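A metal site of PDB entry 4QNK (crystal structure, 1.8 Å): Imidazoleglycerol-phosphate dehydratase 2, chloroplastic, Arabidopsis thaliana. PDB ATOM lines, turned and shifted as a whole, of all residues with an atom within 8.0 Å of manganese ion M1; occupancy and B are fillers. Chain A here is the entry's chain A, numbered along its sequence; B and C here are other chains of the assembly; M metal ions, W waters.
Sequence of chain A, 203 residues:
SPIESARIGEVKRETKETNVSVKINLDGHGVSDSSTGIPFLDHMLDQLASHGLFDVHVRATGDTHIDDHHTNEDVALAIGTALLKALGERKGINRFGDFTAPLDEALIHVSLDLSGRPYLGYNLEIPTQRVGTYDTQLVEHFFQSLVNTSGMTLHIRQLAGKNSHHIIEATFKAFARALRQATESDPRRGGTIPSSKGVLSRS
The side-chain amide oxygen of Asn 163 of chain B lies within hydrogen-bond range of the backbone NH of His 166 of chain B (3.0 Å). OE1 of Glu 105 of chain B sits at hydrogen-bond distance from ND1 of His 166 of chain B (2.8 Å). A ring nitrogen (ND1) of His 141 lies within hydrogen-bond range of the side-chain hydroxyl (OG) of Ser 145 (3.1 Å).
Of the 17 residues printed, 4 come within 4 Å of manganese ion M1.
Manganese ion M1 is bound by water W2, water W1, the side-chain carboxylate (OE1) of Glu 73, a ring nitrogen (NE2) of His 166 of chain B, a ring nitrogen (NE2) of His 69 and a ring nitrogen (NE2) of His 141.
Water W2 lies within hydrogen-bond range of OD2 of Asp 104 of chain B (2.6 Å), OE2 of Glu 73 (2.7 Å) and NE of Arg 117 of chain C (3.5 Å).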
ATOM      1  N   HIS A  69       3.247  22.320  -0.629  1.00  0.00           N
ATOM      2  CA  HIS A  69       2.795  22.800   0.689  1.00  0.00           C
ATOM      3  C   HIS A  69       3.811  23.699   1.398  1.00  0.00           C
ATOM      4  O   HIS A  69       3.457  24.807   1.823  1.00  0.00           O
ATOM      5  CB  HIS A  69       2.495  21.594   1.572  1.00  0.00           C
ATOM      6  CG  HIS A  69       1.830  21.922   2.859  1.00  0.00           C
ATOM      7  ND1 HIS A  69       0.567  21.482   3.167  1.00  0.00           N
ATOM      8  CD2 HIS A  69       2.282  22.567   3.956  1.00  0.00           C
ATOM      9  CE1 HIS A  69       0.271  21.835   4.404  1.00  0.00           C
ATOM     10  NE2 HIS A  69       1.278  22.549   4.884  1.00  0.00           N
ATOM     11  N   HIS A  70       5.085  23.249   1.521  1.00  0.00           N
ATOM     12  CA  HIS A  70       6.067  23.992   2.344  1.00  0.00           C
ATOM     13  C   HIS A  70       6.356  25.347   1.690  1.00  0.00           C
ATOM     14  O   HIS A  70       6.392  26.369   2.377  1.00  0.00           O
ATOM     15  CB  HIS A  70       7.371  23.196   2.577  1.00  0.00           C
ATOM     16  CG  HIS A  70       7.166  21.877   3.245  1.00  0.00           C
ATOM     17  ND1 HIS A  70       8.050  20.833   3.104  1.00  0.00           N
ATOM     18  CD2 HIS A  70       6.191  21.427   4.057  1.00  0.00           C
ATOM     19  CE1 HIS A  70       7.595  19.778   3.772  1.00  0.00           C
ATOM     20  NE2 HIS A  70       6.503  20.144   4.397  1.00  0.00           N
ATOM     21  N   ASN A  72       4.364  27.070  -0.432  1.00  0.00           N
ATOM     22  CA  ASN A  72       3.140  27.900  -0.379  1.00  0.00           C
ATOM     23  C   ASN A  72       3.021  28.589   0.990  1.00  0.00           C
ATOM     24  O   ASN A  72       2.725  29.780   1.124  1.00  0.00           O
ATOM     25  CB  ASN A  72       1.974  26.995  -0.665  1.00  0.00           C
ATOM     26  CG  ASN A  72       0.629  27.713  -0.681  1.00  0.00           C
ATOM     27  OD1 ASN A  72       0.286  28.381  -1.659  1.00  0.00           O
ATOM     28  ND2 ASN A  72      -0.143  27.522   0.372  1.00  0.00           N
ATOM     29  N   GLU A  73       3.282  27.816   2.038  1.00  0.00           N
ATOM     30  CA  GLU A  73       3.179  28.300   3.397  1.00  0.00           C
ATOM     31  C   GLU A  73       4.245  29.346   3.678  1.00  0.00           C
ATOM     32  O   GLU A  73       3.989  30.392   4.240  1.00  0.00           O
ATOM     33  CB  GLU A  73       3.346  27.119   4.378  1.00  0.00           C
ATOM     34  CG  GLU A  73       3.369  27.509   5.817  1.00  0.00           C
ATOM     35  CD  GLU A  73       3.067  26.355   6.768  1.00  0.00           C
ATOM     36  OE1 GLU A  73       2.777  25.208   6.297  1.00  0.00           O
ATOM     37  OE2 GLU A  73       3.087  26.630   7.995  1.00  0.00           O
ATOM     38  N   ASP A  74       5.471  29.031   3.313  1.00  0.00           N
ATOM     39  CA  ASP A  74       6.608  29.914   3.605  1.00  0.00           C
ATOM     40  C   ASP A  74       6.515  31.268   2.848  1.00  0.00           C
ATOM     41  O   ASP A  74       6.863  32.298   3.395  1.00  0.00           O
ATOM     42  CB  ASP A  74       7.953  29.187   3.405  1.00  0.00           C
ATOM     43  CG  ASP A  74       8.294  28.203   4.585  1.00  0.00           C
ATOM     44  OD1 ASP A  74       7.756  28.352   5.707  1.00  0.00           O
ATOM     45  OD2 ASP A  74       9.088  27.247   4.367  1.00  0.00           O
ATOM     46  N   LEU A  77       3.678  33.248   4.720  1.00  0.00           N
ATOM     47  CA  LEU A  77       4.218  33.772   5.973  1.00  0.00           C
ATOM     48  C   LEU A  77       5.086  35.014   5.745  1.00  0.00           C
ATOM     49  O   LEU A  77       4.905  36.040   6.426  1.00  0.00           O
ATOM     50  CB  LEU A  77       4.979  32.699   6.760  1.00  0.00           C
ATOM     51  CG  LEU A  77       4.185  31.491   7.263  1.00  0.00           C
ATOM     52  CD1 LEU A  77       5.163  30.360   7.660  1.00  0.00           C
ATOM     53  CD2 LEU A  77       3.209  31.850   8.411  1.00  0.00           C
ATOM     54  N   LEU A 138      -4.416  24.384  -0.817  1.00  0.00           N
ATOM     55  CA  LEU A 138      -3.369  25.368  -0.449  1.00  0.00           C
ATOM     56  C   LEU A 138      -3.863  26.818  -0.454  1.00  0.00           C
ATOM     57  O   LEU A 138      -3.189  27.691   0.098  1.00  0.00           O
ATOM     58  CB  LEU A 138      -2.128  25.195  -1.311  1.00  0.00           C
ATOM     59  CG  LEU A 138      -1.521  23.810  -1.171  1.00  0.00           C
ATOM     60  CD1 LEU A 138      -0.354  23.635  -2.131  1.00  0.00           C
ATOM     61  CD2 LEU A 138      -1.076  23.501   0.251  1.00  0.00           C
ATOM     62  N   HIS A 141      -4.706  27.644   3.127  1.00  0.00           N
ATOM     63  CA  HIS A 141      -3.464  27.680   3.882  1.00  0.00           C
ATOM     64  C   HIS A 141      -2.664  28.976   3.572  1.00  0.00           C
ATOM     65  O   HIS A 141      -2.014  29.559   4.459  1.00  0.00           O
ATOM     66  CB  HIS A 141      -2.585  26.460   3.608  1.00  0.00           C
ATOM     67  CG  HIS A 141      -1.655  26.121   4.725  1.00  0.00           C
ATOM     68  ND1 HIS A 141      -0.971  27.069   5.451  1.00  0.00           N
ATOM     69  CD2 HIS A 141      -1.214  24.928   5.170  1.00  0.00           C
ATOM     70  CE1 HIS A 141      -0.210  26.464   6.348  1.00  0.00           C
ATOM     71  NE2 HIS A 141      -0.298  25.163   6.163  1.00  0.00           N
ATOM     72  N   SER A 145      -1.865  31.540   6.701  1.00  0.00           N
ATOM     73  CA  SER A 145      -0.471  31.869   6.999  1.00  0.00           C
ATOM     74  C   SER A 145      -0.208  33.389   6.895  1.00  0.00           C
ATOM     75  O   SER A 145       0.437  34.017   7.754  1.00  0.00           O
ATOM     76  CB  SER A 145       0.480  31.062   6.106  1.00  0.00           C
ATOM     77  OG  SER A 145       0.399  29.673   6.441  1.00  0.00           O
ATOM     78  N   LEU B 103      -0.945  19.109  14.472  1.00  0.00           N
ATOM     79  CA  LEU B 103      -0.230  19.857  13.451  1.00  0.00           C
ATOM     80  C   LEU B 103      -1.278  20.868  12.909  1.00  0.00           C
ATOM     81  O   LEU B 103      -2.167  20.514  12.128  1.00  0.00           O
ATOM     82  CB  LEU B 103       0.361  18.978  12.337  1.00  0.00           C
ATOM     83  CG  LEU B 103       1.442  19.638  11.488  1.00  0.00           C
ATOM     84  CD1 LEU B 103       1.881  18.716  10.339  1.00  0.00           C
ATOM     85  CD2 LEU B 103       1.092  20.975  10.929  1.00  0.00           C
ATOM     86  N   ASP B 104      -1.190  22.094  13.411  1.00  0.00           N
ATOM     87  CA  ASP B 104      -2.157  23.152  13.156  1.00  0.00           C
ATOM     88  C   ASP B 104      -3.548  22.598  13.446  1.00  0.00           C
ATOM     89  O   ASP B 104      -3.774  22.172  14.568  1.00  0.00           O
ATOM     90  CB  ASP B 104      -2.043  23.686  11.722  1.00  0.00           C
ATOM     91  CG  ASP B 104      -0.740  24.436  11.456  1.00  0.00           C
ATOM     92  OD1 ASP B 104       0.071  24.651  12.399  1.00  0.00           O
ATOM     93  OD2 ASP B 104      -0.534  24.815  10.270  1.00  0.00           O
ATOM     94  N   GLU B 105      -4.450  22.561  12.455  1.00  0.00           N
ATOM     95  CA  GLU B 105      -5.836  22.094  12.699  1.00  0.00           C
ATOM     96  C   GLU B 105      -6.011  20.576  12.908  1.00  0.00           C
ATOM     97  O   GLU B 105      -7.052  20.134  13.444  1.00  0.00           O
ATOM     98  CB  GLU B 105      -6.791  22.623  11.596  1.00  0.00           C
ATOM     99  CG  GLU B 105      -7.011  21.734  10.380  1.00  0.00           C
ATOM    100  CD  GLU B 105      -5.742  21.343   9.636  1.00  0.00           C
ATOM    101  OE1 GLU B 105      -4.735  22.111   9.671  1.00  0.00           O
ATOM    102  OE2 GLU B 105      -5.790  20.270   8.945  1.00  0.00           O
ATOM    103  N   ASN B 163      -6.524  19.573   6.250  1.00  0.00           N
ATOM    104  CA  ASN B 163      -5.483  19.526   5.235  1.00  0.00           C
ATOM    105  C   ASN B 163      -4.832  18.131   5.199  1.00  0.00           C
ATOM    106  O   ASN B 163      -4.384  17.632   6.242  1.00  0.00           O
ATOM    107  CB  ASN B 163      -4.455  20.577   5.529  1.00  0.00           C
ATOM    108  CG  ASN B 163      -3.332  20.604   4.506  1.00  0.00           C
ATOM    109  OD1 ASN B 163      -2.424  19.748   4.538  1.00  0.00           O
ATOM    110  ND2 ASN B 163      -3.365  21.591   3.612  1.00  0.00           N
ATOM    111  N   HIS B 165      -1.984  16.815   3.970  1.00  0.00           N
ATOM    112  CA  HIS B 165      -0.558  16.812   4.362  1.00  0.00           C
ATOM    113  C   HIS B 165      -0.479  16.928   5.903  1.00  0.00           C
ATOM    114  O   HIS B 165       0.235  16.167   6.545  1.00  0.00           O
ATOM    115  CB  HIS B 165       0.143  17.975   3.634  1.00  0.00           C
ATOM    116  CG  HIS B 165       1.638  18.004   3.752  1.00  0.00           C
ATOM    117  ND1 HIS B 165       2.455  18.331   2.689  1.00  0.00           N
ATOM    118  CD2 HIS B 165       2.457  17.879   4.826  1.00  0.00           C
ATOM    119  CE1 HIS B 165       3.716  18.339   3.090  1.00  0.00           C
ATOM    120  NE2 HIS B 165       3.752  18.107   4.387  1.00  0.00           N
ATOM    121  N   HIS B 166      -1.273  17.819   6.501  1.00  0.00           N
ATOM    122  CA  HIS B 166      -1.284  17.966   7.961  1.00  0.00           C
ATOM    123  C   HIS B 166      -1.781  16.696   8.657  1.00  0.00           C
ATOM    124  O   HIS B 166      -1.180  16.239   9.630  1.00  0.00           O
ATOM    125  CB  HIS B 166      -2.127  19.145   8.472  1.00  0.00           C
ATOM    126  CG  HIS B 166      -1.566  20.492   8.162  1.00  0.00           C
ATOM    127  ND1 HIS B 166      -2.255  21.668   8.407  1.00  0.00           N
ATOM    128  CD2 HIS B 166      -0.400  20.860   7.598  1.00  0.00           C
ATOM    129  CE1 HIS B 166      -1.532  22.692   7.988  1.00  0.00           C
ATOM    130  NE2 HIS B 166      -0.376  22.224   7.540  1.00  0.00           N
ATOM    131  N   GLU B 169       1.004  13.954   8.271  1.00  0.00           N
ATOM    132  CA  GLU B 169       2.225  14.305   8.973  1.00  0.00           C
ATOM    133  C   GLU B 169       1.999  14.238  10.497  1.00  0.00           C
ATOM    134  O   GLU B 169       2.844  13.723  11.219  1.00  0.00           O
ATOM    135  CB  GLU B 169       2.729  15.679   8.559  1.00  0.00           C
ATOM    136  CG  GLU B 169       4.053  16.042   9.199  1.00  0.00           C
ATOM    137  CD  GLU B 169       4.701  17.269   8.550  1.00  0.00           C
ATOM    138  OE1 GLU B 169       4.649  17.370   7.318  1.00  0.00           O
ATOM    139  OE2 GLU B 169       5.253  18.116   9.276  1.00  0.00           O
ATOM    140  N   ARG C 117       3.247  28.556  15.341  1.00  0.00           N
ATOM    141  CA  ARG C 117       2.099  28.826  14.472  1.00  0.00           C
ATOM    142  C   ARG C 117       0.829  28.852  15.286  1.00  0.00           C
ATOM    143  O   ARG C 117       0.431  27.800  15.804  1.00  0.00           O
ATOM    144  CB  ARG C 117       1.967  27.754  13.384  1.00  0.00           C
ATOM    145  CG  ARG C 117       3.188  27.612  12.486  1.00  0.00           C
ATOM    146  CD  ARG C 117       2.981  26.538  11.406  1.00  0.00           C
ATOM    147  NE  ARG C 117       2.781  25.222  12.039  1.00  0.00           N
ATOM    148  CZ  ARG C 117       3.762  24.391  12.386  1.00  0.00           C
ATOM    149  NH1 ARG C 117       5.033  24.674  12.098  1.00  0.00           N
ATOM    150  NH2 ARG C 117       3.478  23.266  12.985  1.00  0.00           N
HETATM  151 MN    MN M   1       1.264  23.635   6.881  1.00  0.00          MN
HETATM  152 MN    MN M   2       5.544  18.601   5.739  1.00  0.00          MN
HETATM  153  O   HOH W   1       2.965  22.309   7.344  1.00  0.00           O
HETATM  154  O   HOH W   2       1.573  24.509   8.849  1.00  0.00           O
